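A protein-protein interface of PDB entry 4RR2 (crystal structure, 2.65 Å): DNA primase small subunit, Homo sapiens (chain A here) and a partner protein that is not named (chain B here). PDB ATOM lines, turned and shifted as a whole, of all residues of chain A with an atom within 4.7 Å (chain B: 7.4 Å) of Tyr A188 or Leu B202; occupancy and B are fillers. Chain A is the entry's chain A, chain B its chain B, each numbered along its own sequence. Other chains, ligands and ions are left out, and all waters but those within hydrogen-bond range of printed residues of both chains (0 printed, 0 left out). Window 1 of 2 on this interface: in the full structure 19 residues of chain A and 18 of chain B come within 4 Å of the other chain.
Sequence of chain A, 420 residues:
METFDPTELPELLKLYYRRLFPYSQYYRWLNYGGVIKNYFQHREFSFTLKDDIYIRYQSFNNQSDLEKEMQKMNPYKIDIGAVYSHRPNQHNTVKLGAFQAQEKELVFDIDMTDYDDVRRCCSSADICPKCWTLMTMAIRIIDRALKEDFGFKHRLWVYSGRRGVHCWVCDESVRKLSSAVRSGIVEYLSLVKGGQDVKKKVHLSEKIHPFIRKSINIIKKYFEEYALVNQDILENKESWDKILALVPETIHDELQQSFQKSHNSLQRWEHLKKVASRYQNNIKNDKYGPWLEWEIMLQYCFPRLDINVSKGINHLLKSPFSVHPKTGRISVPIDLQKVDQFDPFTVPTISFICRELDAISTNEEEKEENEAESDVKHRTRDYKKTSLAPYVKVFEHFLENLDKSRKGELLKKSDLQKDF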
ATOM      1  N   ALA A 145     -18.538  33.434 -18.224  1.00  0.00           N
ATOM      2  CA  ALA A 145     -17.953  32.659 -17.131  1.00  0.00           C
ATOM      3  C   ALA A 145     -16.947  33.518 -16.363  1.00  0.00           C
ATOM      4  O   ALA A 145     -17.020  33.643 -15.149  1.00  0.00           O
ATOM      5  CB  ALA A 145     -17.268  31.423 -17.684  1.00  0.00           C
ATOM      6  N   ASP A 149     -19.026  33.840 -13.201  1.00  0.00           N
ATOM      7  CA  ASP A 149     -18.526  32.731 -12.402  1.00  0.00           C
ATOM      8  C   ASP A 149     -17.339  33.113 -11.532  1.00  0.00           C
ATOM      9  O   ASP A 149     -17.376  32.953 -10.317  1.00  0.00           O
ATOM     10  CB  ASP A 149     -18.101  31.584 -13.304  1.00  0.00           C
ATOM     11  CG  ASP A 149     -19.262  30.966 -14.019  1.00  0.00           C
ATOM     12  OD1 ASP A 149     -20.338  31.593 -14.006  1.00  0.00           O
ATOM     13  OD2 ASP A 149     -19.099  29.866 -14.595  1.00  0.00           O
ATOM     14  N   PHE A 150     -16.292  33.625 -12.163  1.00  0.00           N
ATOM     15  CA  PHE A 150     -15.084  33.977 -11.452  1.00  0.00           C
ATOM     16  C   PHE A 150     -15.038  35.370 -10.867  1.00  0.00           C
ATOM     17  O   PHE A 150     -14.147  35.682 -10.075  1.00  0.00           O
ATOM     18  CB  PHE A 150     -13.882  33.735 -12.360  1.00  0.00           C
ATOM     19  CG  PHE A 150     -13.755  32.311 -12.789  1.00  0.00           C
ATOM     20  CD1 PHE A 150     -14.233  31.894 -14.012  1.00  0.00           C
ATOM     21  CD2 PHE A 150     -13.212  31.369 -11.931  1.00  0.00           C
ATOM     22  CE1 PHE A 150     -14.168  30.552 -14.378  1.00  0.00           C
ATOM     23  CE2 PHE A 150     -13.146  30.038 -12.289  1.00  0.00           C
ATOM     24  CZ  PHE A 150     -13.627  29.629 -13.510  1.00  0.00           C
ATOM     25  N   GLY A 184      -6.557  25.431 -13.957  1.00  0.00           N
ATOM     26  CA  GLY A 184      -7.859  24.980 -13.486  1.00  0.00           C
ATOM     27  C   GLY A 184      -9.012  25.744 -14.107  1.00  0.00           C
ATOM     28  O   GLY A 184     -10.052  25.176 -14.426  1.00  0.00           O
ATOM     29  N   ILE A 185      -8.825  27.047 -14.261  1.00  0.00           N
ATOM     30  CA  ILE A 185      -9.827  27.882 -14.873  1.00  0.00           C
ATOM     31  C   ILE A 185     -10.065  27.349 -16.279  1.00  0.00           C
ATOM     32  O   ILE A 185     -11.209  27.211 -16.709  1.00  0.00           O
ATOM     33  CB  ILE A 185      -9.349  29.328 -14.945  1.00  0.00           C
ATOM     34  CG1 ILE A 185      -9.306  29.903 -13.526  1.00  0.00           C
ATOM     35  CG2 ILE A 185     -10.239  30.130 -15.883  1.00  0.00           C
ATOM     36  CD1 ILE A 185      -8.960  31.376 -13.447  1.00  0.00           C
ATOM     37  N   VAL A 186      -8.988  27.023 -16.984  1.00  0.00           N
ATOM     38  CA  VAL A 186      -9.115  26.508 -18.331  1.00  0.00           C
ATOM     39  C   VAL A 186      -9.883  25.196 -18.382  1.00  0.00           C
ATOM     40  O   VAL A 186     -10.713  25.003 -19.260  1.00  0.00           O
ATOM     41  CB  VAL A 186      -7.736  26.316 -19.003  1.00  0.00           C
ATOM     42  CG1 VAL A 186      -7.902  25.589 -20.344  1.00  0.00           C
ATOM     43  CG2 VAL A 186      -7.084  27.676 -19.241  1.00  0.00           C
ATOM     44  N   GLU A 187      -9.608  24.295 -17.448  1.00  0.00           N
ATOM     45  CA  GLU A 187     -10.293  23.003 -17.406  1.00  0.00           C
ATOM     46  C   GLU A 187     -11.785  23.178 -17.100  1.00  0.00           C
ATOM     47  O   GLU A 187     -12.626  22.395 -17.539  1.00  0.00           O
ATOM     48  CB  GLU A 187      -9.692  22.126 -16.311  1.00  0.00           C
ATOM     49  CG  GLU A 187      -8.467  21.312 -16.677  1.00  0.00           C
ATOM     50  CD  GLU A 187      -7.962  20.522 -15.481  1.00  0.00           C
ATOM     51  OE1 GLU A 187      -7.046  21.015 -14.782  1.00  0.00           O
ATOM     52  OE2 GLU A 187      -8.506  19.418 -15.230  1.00  0.00           O
ATOM     53  N   TYR A 188     -12.099  24.199 -16.316  1.00  0.00           N
ATOM     54  CA  TYR A 188     -13.460  24.468 -15.935  1.00  0.00           C
ATOM     55  C   TYR A 188     -14.291  24.944 -17.114  1.00  0.00           C
ATOM     56  O   TYR A 188     -15.493  24.699 -17.158  1.00  0.00           O
ATOM     57  CB  TYR A 188     -13.468  25.523 -14.848  1.00  0.00           C
ATOM     58  CG  TYR A 188     -14.829  26.099 -14.550  1.00  0.00           C
ATOM     59  CD1 TYR A 188     -15.748  25.409 -13.766  1.00  0.00           C
ATOM     60  CD2 TYR A 188     -15.177  27.362 -15.010  1.00  0.00           C
ATOM     61  CE1 TYR A 188     -16.975  25.976 -13.438  1.00  0.00           C
ATOM     62  CE2 TYR A 188     -16.393  27.935 -14.690  1.00  0.00           C
ATOM     63  CZ  TYR A 188     -17.283  27.243 -13.902  1.00  0.00           C
ATOM     64  OH  TYR A 188     -18.458  27.851 -13.549  1.00  0.00           O
ATOM     65  N   LEU A 189     -13.636  25.629 -18.051  1.00  0.00           N
ATOM     66  CA  LEU A 189     -14.259  26.182 -19.255  1.00  0.00           C
ATOM     67  C   LEU A 189     -14.188  25.212 -20.423  1.00  0.00           C
ATOM     68  O   LEU A 189     -14.878  25.393 -21.410  1.00  0.00           O
ATOM     69  CB  LEU A 189     -13.541  27.454 -19.709  1.00  0.00           C
ATOM     70  CG  LEU A 189     -13.426  28.664 -18.784  1.00  0.00           C
ATOM     71  CD1 LEU A 189     -12.432  29.666 -19.391  1.00  0.00           C
ATOM     72  CD2 LEU A 189     -14.799  29.279 -18.560  1.00  0.00           C
ATOM     73  N   SER A 190     -13.337  24.202 -20.319  1.00  0.00           N
ATOM     74  CA  SER A 190     -13.164  23.247 -21.392  1.00  0.00           C
ATOM     75  C   SER A 190     -14.231  22.182 -21.407  1.00  0.00           C
ATOM     76  O   SER A 190     -14.660  21.693 -20.356  1.00  0.00           O
ATOM     77  CB  SER A 190     -11.785  22.607 -21.302  1.00  0.00           C
ATOM     78  OG  SER A 190     -10.800  23.547 -21.663  1.00  0.00           O
ATOM     79  N   HIS A 209     -23.990  20.750 -15.208  1.00  0.00           N
ATOM     80  CA  HIS A 209     -23.424  21.855 -14.448  1.00  0.00           C
ATOM     81  C   HIS A 209     -23.911  23.179 -15.036  1.00  0.00           C
ATOM     82  O   HIS A 209     -23.943  23.347 -16.253  1.00  0.00           O
ATOM     83  CB  HIS A 209     -21.884  21.791 -14.488  1.00  0.00           C
ATOM     84  CG  HIS A 209     -21.219  22.770 -13.574  1.00  0.00           C
ATOM     85  ND1 HIS A 209     -21.258  24.132 -13.786  1.00  0.00           N
ATOM     86  CD2 HIS A 209     -20.551  22.593 -12.410  1.00  0.00           C
ATOM     87  CE1 HIS A 209     -20.649  24.752 -12.792  1.00  0.00           C
ATOM     88  NE2 HIS A 209     -20.211  23.840 -11.943  1.00  0.00           N
ATOM     89  N   PHE A 211     -22.605  26.001 -15.677  1.00  0.00           N
ATOM     90  CA  PHE A 211     -21.752  26.656 -16.659  1.00  0.00           C
ATOM     91  C   PHE A 211     -22.078  26.064 -18.007  1.00  0.00           C
ATOM     92  O   PHE A 211     -22.151  26.769 -18.997  1.00  0.00           O
ATOM     93  CB  PHE A 211     -20.254  26.454 -16.329  1.00  0.00           C
ATOM     94  CG  PHE A 211     -19.334  26.705 -17.504  1.00  0.00           C
ATOM     95  CD1 PHE A 211     -18.959  25.670 -18.341  1.00  0.00           C
ATOM     96  CD2 PHE A 211     -18.906  27.979 -17.806  1.00  0.00           C
ATOM     97  CE1 PHE A 211     -18.168  25.911 -19.461  1.00  0.00           C
ATOM     98  CE2 PHE A 211     -18.122  28.217 -18.920  1.00  0.00           C
ATOM     99  CZ  PHE A 211     -17.757  27.185 -19.746  1.00  0.00           C
ATOM    100  N   ARG B 162     -30.013  29.312  -4.290  1.00  0.00           N
ATOM    101  CA  ARG B 162     -28.961  28.640  -5.044  1.00  0.00           C
ATOM    102  C   ARG B 162     -29.030  27.126  -4.954  1.00  0.00           C
ATOM    103  O   ARG B 162     -28.282  26.423  -5.630  1.00  0.00           O
ATOM    104  CB  ARG B 162     -27.585  29.121  -4.582  1.00  0.00           C
ATOM    105  CG  ARG B 162     -27.086  30.317  -5.361  1.00  0.00           C
ATOM    106  CD  ARG B 162     -25.674  30.661  -4.968  1.00  0.00           C
ATOM    107  NE  ARG B 162     -25.652  31.476  -3.768  1.00  0.00           N
ATOM    108  CZ  ARG B 162     -26.026  32.744  -3.745  1.00  0.00           C
ATOM    109  NH1 ARG B 162     -26.443  33.324  -4.858  1.00  0.00           N
ATOM    110  NH2 ARG B 162     -25.981  33.430  -2.615  1.00  0.00           N
ATOM    111  N   GLU B 165     -28.883  25.539  -8.350  1.00  0.00           N
ATOM    112  CA  GLU B 165     -27.559  25.507  -8.971  1.00  0.00           C
ATOM    113  C   GLU B 165     -26.680  24.480  -8.281  1.00  0.00           C
ATOM    114  O   GLU B 165     -26.206  23.524  -8.904  1.00  0.00           O
ATOM    115  CB  GLU B 165     -26.902  26.887  -8.868  1.00  0.00           C
ATOM    116  CG  GLU B 165     -27.737  28.005  -9.463  1.00  0.00           C
ATOM    117  CD  GLU B 165     -27.929  27.860 -10.963  1.00  0.00           C
ATOM    118  OE1 GLU B 165     -28.439  26.810 -11.415  1.00  0.00           O
ATOM    119  OE2 GLU B 165     -27.572  28.803 -11.695  1.00  0.00           O
ATOM    120  N   SER B 169     -24.396  21.354  -9.672  1.00  0.00           N
ATOM    121  CA  SER B 169     -22.939  21.411  -9.738  1.00  0.00           C
ATOM    122  C   SER B 169     -22.315  20.129  -9.167  1.00  0.00           C
ATOM    123  O   SER B 169     -21.349  19.590  -9.711  1.00  0.00           O
ATOM    124  CB  SER B 169     -22.430  22.624  -8.946  1.00  0.00           C
ATOM    125  OG  SER B 169     -23.141  23.811  -9.272  1.00  0.00           O
ATOM    126  N   ILE B 186     -16.563  30.081  -0.117  1.00  0.00           N
ATOM    127  CA  ILE B 186     -15.118  30.271  -0.067  1.00  0.00           C
ATOM    128  C   ILE B 186     -14.533  30.696  -1.410  1.00  0.00           C
ATOM    129  O   ILE B 186     -15.058  30.339  -2.464  1.00  0.00           O
ATOM    130  CB  ILE B 186     -14.407  28.971   0.376  1.00  0.00           C
ATOM    131  CG1 ILE B 186     -14.457  27.920  -0.731  1.00  0.00           C
ATOM    132  CG2 ILE B 186     -15.110  28.396   1.569  1.00  0.00           C
ATOM    133  CD1 ILE B 186     -13.763  26.636  -0.372  1.00  0.00           C
ATOM    134  N   PRO B 187     -13.438  31.484  -1.385  1.00  0.00           N
ATOM    135  CA  PRO B 187     -12.764  31.962  -2.589  1.00  0.00           C
ATOM    136  C   PRO B 187     -12.575  30.820  -3.568  1.00  0.00           C
ATOM    137  O   PRO B 187     -12.065  29.758  -3.216  1.00  0.00           O
ATOM    138  CB  PRO B 187     -11.447  32.487  -2.045  1.00  0.00           C
ATOM    139  CG  PRO B 187     -11.875  33.116  -0.791  1.00  0.00           C
ATOM    140  CD  PRO B 187     -12.787  32.052  -0.191  1.00  0.00           C
ATOM    141  N   PHE B 188     -12.988  31.056  -4.806  1.00  0.00           N
ATOM    142  CA  PHE B 188     -12.921  30.054  -5.861  1.00  0.00           C
ATOM    143  C   PHE B 188     -11.561  29.403  -6.005  1.00  0.00           C
ATOM    144  O   PHE B 188     -11.468  28.223  -6.329  1.00  0.00           O
ATOM    145  CB  PHE B 188     -13.350  30.682  -7.190  1.00  0.00           C
ATOM    146  CG  PHE B 188     -12.219  31.209  -8.018  1.00  0.00           C
ATOM    147  CD1 PHE B 188     -11.485  30.358  -8.834  1.00  0.00           C
ATOM    148  CD2 PHE B 188     -11.929  32.563  -8.033  1.00  0.00           C
ATOM    149  CE1 PHE B 188     -10.483  30.860  -9.662  1.00  0.00           C
ATOM    150  CE2 PHE B 188     -10.928  33.075  -8.854  1.00  0.00           C
ATOM    151  CZ  PHE B 188     -10.207  32.219  -9.671  1.00  0.00           C
ATOM    152  N   ALA B 189     -10.501  30.163  -5.767  1.00  0.00           N
ATOM    153  CA  ALA B 189      -9.180  29.587  -5.908  1.00  0.00           C
ATOM    154  C   ALA B 189      -9.010  28.469  -4.883  1.00  0.00           C
ATOM    155  O   ALA B 189      -8.601  27.353  -5.216  1.00  0.00           O
ATOM    156  CB  ALA B 189      -8.128  30.651  -5.725  1.00  0.00           C
ATOM    157  N   ALA B 191     -10.847  26.448  -3.890  1.00  0.00           N
ATOM    158  CA  ALA B 191     -11.547  25.212  -4.229  1.00  0.00           C
ATOM    159  C   ALA B 191     -11.014  24.556  -5.491  1.00  0.00           C
ATOM    160  O   ALA B 191     -11.649  23.676  -6.059  1.00  0.00           O
ATOM    161  CB  ALA B 191     -13.017  25.480  -4.373  1.00  0.00           C
ATOM    162  N   LEU B 194     -11.882  21.255  -6.784  1.00  0.00           N
ATOM    163  CA  LEU B 194     -13.303  21.029  -6.979  1.00  0.00           C
ATOM    164  C   LEU B 194     -13.819  21.632  -8.296  1.00  0.00           C
ATOM    165  O   LEU B 194     -14.399  20.928  -9.128  1.00  0.00           O
ATOM    166  CB  LEU B 194     -14.100  21.605  -5.807  1.00  0.00           C
ATOM    167  CG  LEU B 194     -14.093  20.787  -4.515  1.00  0.00           C
ATOM    168  CD1 LEU B 194     -15.085  21.393  -3.532  1.00  0.00           C
ATOM    169  CD2 LEU B 194     -14.444  19.337  -4.823  1.00  0.00           C
ATOM    170  N   PHE B 195     -13.582  22.925  -8.495  1.00  0.00           N
ATOM    171  CA  PHE B 195     -14.069  23.600  -9.686  1.00  0.00           C
ATOM    172  C   PHE B 195     -13.424  23.243 -11.019  1.00  0.00           C
ATOM    173  O   PHE B 195     -14.047  23.402 -12.053  1.00  0.00           O
ATOM    174  CB  PHE B 195     -14.029  25.121  -9.471  1.00  0.00           C
ATOM    175  CG  PHE B 195     -12.708  25.774  -9.808  1.00  0.00           C
ATOM    176  CD1 PHE B 195     -12.235  25.811 -11.117  1.00  0.00           C
ATOM    177  CD2 PHE B 195     -11.990  26.459  -8.832  1.00  0.00           C
ATOM    178  CE1 PHE B 195     -11.071  26.530 -11.442  1.00  0.00           C
ATOM    179  CE2 PHE B 195     -10.831  27.178  -9.154  1.00  0.00           C
ATOM    180  CZ  PHE B 195     -10.377  27.216 -10.454  1.00  0.00           C
ATOM    181  N   ARG B 196     -12.184  22.776 -11.016  1.00  0.00           N
ATOM    182  CA  ARG B 196     -11.521  22.438 -12.268  1.00  0.00           C
ATOM    183  C   ARG B 196     -12.174  21.233 -12.909  1.00  0.00           C
ATOM    184  O   ARG B 196     -11.879  20.898 -14.054  1.00  0.00           O
ATOM    185  CB  ARG B 196     -10.028  22.157 -12.040  1.00  0.00           C
ATOM    186  CG  ARG B 196      -9.716  21.105 -10.978  1.00  0.00           C
ATOM    187  CD  ARG B 196      -8.233  20.768 -10.918  1.00  0.00           C
ATOM    188  NE  ARG B 196      -7.826  19.821 -11.951  1.00  0.00           N
ATOM    189  CZ  ARG B 196      -7.420  18.573 -11.709  1.00  0.00           C
ATOM    190  NH1 ARG B 196      -7.368  18.120 -10.463  1.00  0.00           N
ATOM    191  NH2 ARG B 196      -7.058  17.774 -12.712  1.00  0.00           N
ATOM    192  N   GLY B 197     -13.037  20.565 -12.156  1.00  0.00           N
ATOM    193  CA  GLY B 197     -13.731  19.398 -12.673  1.00  0.00           C
ATOM    194  C   GLY B 197     -15.223  19.664 -12.601  1.00  0.00           C
ATOM    195  O   GLY B 197     -16.045  18.759 -12.711  1.00  0.00           O
ATOM    196  N   ARG B 198     -15.564  20.934 -12.419  1.00  0.00           N
ATOM    197  CA  ARG B 198     -16.945  21.354 -12.328  1.00  0.00           C
ATOM    198  C   ARG B 198     -17.694  20.475 -11.345  1.00  0.00           C
ATOM    199  O   ARG B 198     -18.760  19.915 -11.660  1.00  0.00           O
ATOM    200  CB  ARG B 198     -17.616  21.326 -13.714  1.00  0.00           C
ATOM    201  CG  ARG B 198     -17.283  22.529 -14.568  1.00  0.00           C
ATOM    202  CD  ARG B 198     -17.982  22.487 -15.903  1.00  0.00           C
ATOM    203  NE  ARG B 198     -17.167  21.972 -17.002  1.00  0.00           N
ATOM    204  CZ  ARG B 198     -17.213  20.715 -17.410  1.00  0.00           C
ATOM    205  NH1 ARG B 198     -18.039  19.880 -16.800  1.00  0.00           N
ATOM    206  NH2 ARG B 198     -16.439  20.290 -18.403  1.00  0.00           N
ATOM    207  N   LYS B 199     -17.117  20.349 -10.151  1.00  0.00           N
ATOM    208  CA  LYS B 199     -17.738  19.574  -9.088  1.00  0.00           C
ATOM    209  C   LYS B 199     -18.243  20.548  -8.039  1.00  0.00           C
ATOM    210  O   LYS B 199     -18.413  20.181  -6.888  1.00  0.00           O
ATOM    211  CB  LYS B 199     -16.748  18.593  -8.462  1.00  0.00           C
ATOM    212  CG  LYS B 199     -16.278  17.488  -9.394  1.00  0.00           C
ATOM    213  CD  LYS B 199     -15.078  16.774  -8.783  1.00  0.00           C
ATOM    214  CE  LYS B 199     -14.462  15.755  -9.735  1.00  0.00           C
ATOM    215  NZ  LYS B 199     -13.118  15.256  -9.283  1.00  0.00           N
ATOM    216  N   VAL B 200     -18.469  21.793  -8.448  1.00  0.00           N
ATOM    217  CA  VAL B 200     -18.988  22.838  -7.554  1.00  0.00           C
ATOM    218  C   VAL B 200     -19.443  24.114  -8.270  1.00  0.00           C
ATOM    219  O   VAL B 200     -19.023  24.435  -9.379  1.00  0.00           O
ATOM    220  CB  VAL B 200     -17.975  23.293  -6.478  1.00  0.00           C
ATOM    221  CG1 VAL B 200     -17.863  22.257  -5.396  1.00  0.00           C
ATOM    222  CG2 VAL B 200     -16.643  23.588  -7.128  1.00  0.00           C
ATOM    223  N   TYR B 201     -20.268  24.872  -7.576  1.00  0.00           N
ATOM    224  CA  TYR B 201     -20.821  26.062  -8.139  1.00  0.00           C
ATOM    225  C   TYR B 201     -20.053  27.333  -7.807  1.00  0.00           C
ATOM    226  O   TYR B 201     -19.826  27.682  -6.634  1.00  0.00           O
ATOM    227  CB  TYR B 201     -22.305  26.149  -7.728  1.00  0.00           C
ATOM    228  CG  TYR B 201     -23.003  27.408  -8.164  1.00  0.00           C
ATOM    229  CD1 TYR B 201     -23.188  28.458  -7.266  1.00  0.00           C
ATOM    230  CD2 TYR B 201     -23.438  27.574  -9.486  1.00  0.00           C
ATOM    231  CE1 TYR B 201     -23.778  29.642  -7.663  1.00  0.00           C
ATOM    232  CE2 TYR B 201     -24.038  28.770  -9.899  1.00  0.00           C
ATOM    233  CZ  TYR B 201     -24.195  29.803  -8.976  1.00  0.00           C
ATOM    234  OH  TYR B 201     -24.703  31.022  -9.357  1.00  0.00           O
ATOM    235  N   LEU B 202     -19.635  28.000  -8.877  1.00  0.00           N
ATOM    236  CA  LEU B 202     -18.918  29.247  -8.785  1.00  0.00           C
ATOM    237  C   LEU B 202     -19.915  30.331  -9.122  1.00  0.00           C
ATOM    238  O   LEU B 202     -20.739  30.164 -10.010  1.00  0.00           O
ATOM    239  CB  LEU B 202     -17.777  29.305  -9.806  1.00  0.00           C
ATOM    240  CG  LEU B 202     -16.479  28.538  -9.558  1.00  0.00           C
ATOM    241  CD1 LEU B 202     -16.641  27.489  -8.458  1.00  0.00           C
ATOM    242  CD2 LEU B 202     -16.058  27.903 -10.859  1.00  0.00           C
ATOM    243  N   GLU B 203     -19.842  31.437  -8.406  1.00  0.00           N
ATOM    244  CA  GLU B 203     -20.706  32.553  -8.661  1.00  0.00           C
ATOM    245  C   GLU B 203     -20.014  33.769  -8.096  1.00  0.00           C
ATOM    246  O   GLU B 203     -19.917  33.914  -6.889  1.00  0.00           O
ATOM    247  CB  GLU B 203     -22.052  32.386  -7.968  1.00  0.00           C
ATOM    248  CG  GLU B 203     -22.946  33.642  -8.092  1.00  0.00           C
ATOM    249  CD  GLU B 203     -24.198  33.592  -7.222  1.00  0.00           C
ATOM    250  OE1 GLU B 203     -25.084  32.743  -7.488  1.00  0.00           O
ATOM    251  OE2 GLU B 203     -24.284  34.406  -6.266  1.00  0.00           O
ATOM    252  N   ASP B 204     -19.517  34.631  -8.970  1.00  0.00           N
ATOM    253  CA  ASP B 204     -18.871  35.850  -8.534  1.00  0.00           C
ATOM    254  C   ASP B 204     -17.513  35.601  -7.892  1.00  0.00           C
ATOM    255  O   ASP B 204     -17.090  36.357  -7.026  1.00  0.00           O
ATOM    256  CB  ASP B 204     -19.768  36.566  -7.537  1.00  0.00           C
ATOM    257  CG  ASP B 204     -19.422  38.021  -7.394  1.00  0.00           C
ATOM    258  OD1 ASP B 204     -19.835  38.632  -6.386  1.00  0.00           O
ATOM    259  OD2 ASP B 204     -18.750  38.558  -8.301  1.00  0.00           O
ATOM    260  N   GLY B 205     -16.835  34.540  -8.315  1.00  0.00           N
ATOM    261  CA  GLY B 205     -15.525  34.227  -7.770  1.00  0.00           C
ATOM    262  C   GLY B 205     -15.543  33.450  -6.464  1.00  0.00           C
ATOM    263  O   GLY B 205     -14.525  33.362  -5.765  1.00  0.00           O
ATOM    264  N   PHE B 206     -16.701  32.889  -6.133  1.00  0.00           N
ATOM    265  CA  PHE B 206     -16.849  32.119  -4.910  1.00  0.00           C
ATOM    266  C   PHE B 206     -17.346  30.734  -5.202  1.00  0.00           C
ATOM    267  O   PHE B 206     -18.112  30.504  -6.136  1.00  0.00           O
ATOM    268  CB  PHE B 206     -17.809  32.812  -3.944  1.00  0.00           C
ATOM    269  CG  PHE B 206     -17.216  34.007  -3.270  1.00  0.00           C
ATOM    270  CD1 PHE B 206     -16.311  33.850  -2.224  1.00  0.00           C
ATOM    271  CD2 PHE B 206     -17.513  35.292  -3.715  1.00  0.00           C
ATOM    272  CE1 PHE B 206     -15.698  34.969  -1.624  1.00  0.00           C
ATOM    273  CE2 PHE B 206     -16.909  36.420  -3.126  1.00  0.00           C
ATOM    274  CZ  PHE B 206     -15.995  36.254  -2.074  1.00  0.00           C
ATOM    275  N   ALA B 207     -16.884  29.795  -4.398  1.00  0.00           N
ATOM    276  CA  ALA B 207     -17.304  28.428  -4.560  1.00  0.00           C
ATOM    277  C   ALA B 207     -18.284  28.152  -3.422  1.00  0.00           C
ATOM    278  O   ALA B 207     -18.046  28.519  -2.268  1.00  0.00           O
ATOM    279  CB  ALA B 207     -16.102  27.507  -4.489  1.00  0.00           C
ATOM    280  N   TYR B 208     -19.409  27.540  -3.761  1.00  0.00           N
ATOM    281  CA  TYR B 208     -20.417  27.222  -2.771  1.00  0.00           C
ATOM    282  C   TYR B 208     -20.353  25.729  -2.550  1.00  0.00           C
ATOM    283  O   TYR B 208     -20.784  24.945  -3.398  1.00  0.00           O
ATOM    284  CB  TYR B 208     -21.787  27.656  -3.275  1.00  0.00           C
ATOM    285  CG  TYR B 208     -21.958  29.157  -3.276  1.00  0.00           C
ATOM    286  CD1 TYR B 208     -21.869  29.883  -2.098  1.00  0.00           C
ATOM    287  CD2 TYR B 208     -22.230  29.844  -4.448  1.00  0.00           C
ATOM    288  CE1 TYR B 208     -22.052  31.265  -2.084  1.00  0.00           C
ATOM    289  CE2 TYR B 208     -22.417  31.221  -4.453  1.00  0.00           C
ATOM    290  CZ  TYR B 208     -22.329  31.930  -3.269  1.00  0.00           C
ATOM    291  OH  TYR B 208     -22.525  33.297  -3.263  1.00  0.00           O
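Phe A150 touches Phe B188 (CD2 to CE1, 3.6 Å).
CE2 of Phe A150 touches CD2 of Leu B202, at 3.9 Å.
Phe A150 touches Asp B204 (C to C, 3.9 Å).
Phe B195 touches Gly A184.
Arg B196 touches Gly A184 (CA to O, 3.8 Å).
Phe B195 touches Ile A185 (CE1 to N, 3.6 Å).
Phe B195 touches Tyr A188.
Tyr A188 touches Leu B202.
His A209 touches Ser B169 (CD2 to CA, 3.8 Å).
Arg B198 touches His A209.
O of Asp A149 sits at hydrogen-bond distance from N of Glu B203.
N of Asp B204 sits at hydrogen-bond distance from O of Asp A149.
O of Asp A149 is in hydrogen-bond range of N of Gly B205, 2.6 Å away.
The backbone NH (N) of Gly B205 lies close to the backbone carbonyl oxygen (O) of Phe A150.
The guanidinium group of Arg B196 is in salt-bridge range of the side-chain carboxylate of Glu A187.
The guanidinium group (NE) of Arg B198 is in hydrogen-bond range of the backbone carbonyl oxygen (O) of Tyr A188, at 3.2 Å.
NH2 of Arg B198 lies within hydrogen-bond range of O of Ser A190 (3.0 Å).
O of Val B200 lies within hydrogen-bond range of NE2 of His A209 (2.9 Å).
O of Ala A145 sits at hydrogen-bond distance from N of Phe A150.
The side-chain hydroxyl (OG) of Ser A190 sits at hydrogen-bond distance from the backbone carbonyl oxygen (O) of Val A186, 2.8 Å away.
A ring nitrogen (ND1) of His A209 sits at hydrogen-bond distance from the backbone NH (N) of Phe A211, 3.0 Å away.
The guanidinium group (NH1) of Arg B162 is in salt-bridge range of the side-chain carboxylate (OE2) of Glu B203 (2.8 Å).
The backbone carbonyl oxygen (O) of Glu B165 sits at hydrogen-bond distance from the side-chain hydroxyl (OG) of Ser B169 (3.1 Å).
O of Gly B205 is in hydrogen-bond range of N of Phe B188 (2.9 Å).
Of the printed residues of chain B, Tyr A188 touches Phe B195 (3.1 Å), Arg B198 (3.2 Å) and Leu B202 (3.3 Å).
Printed residues of chain B within 4 Å of Ser A190: Arg B198 (3.0 Å).
Of the printed residues of chain A, Ser B169 touches His A209.
Pro B187 touches none of the printed residues of chain A.
Of the printed residues of chain A, Phe B188 touches Phe A150.
Of the printed residues of chain A, Phe B195 touches Gly A184, Ile A185 and Tyr A188.
Printed residues of chain A within 4 Å of Arg B196: Gly A184 (3.8 Å) and Glu A187 (3.2 Å).
Leu B202 touches just these residues of chain A: Asp A149, Phe A150 and Tyr A188.
The nearest printed residue of chain B that does not touch Tyr A188 is Arg B196 (4.01 Å).
The nearest printed residue of chain A that does not touch Leu B202 is His A209 (5.2 Å).
The nearest printed residue of chain B that does not touch Ile A185 is Phe B188 (4.1 Å).
Hydrophobic or aromatic side chains of chain A that line the printed part of chain B: Phe A150, Tyr A188 and His A209.
Hydrophobic or aromatic side chains of chain B within 4 Å of the printed part of chain A: Phe B188, Phe B195 and Leu B202.
Among the printed residues, 19 pairs touch across the chains.
Among the printed residues, Asp or Glu carboxylates within 4 Å of a Lys or Arg side-chain nitrogen of the other chain: Glu A187 with Arg B196 (3.2 Å).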
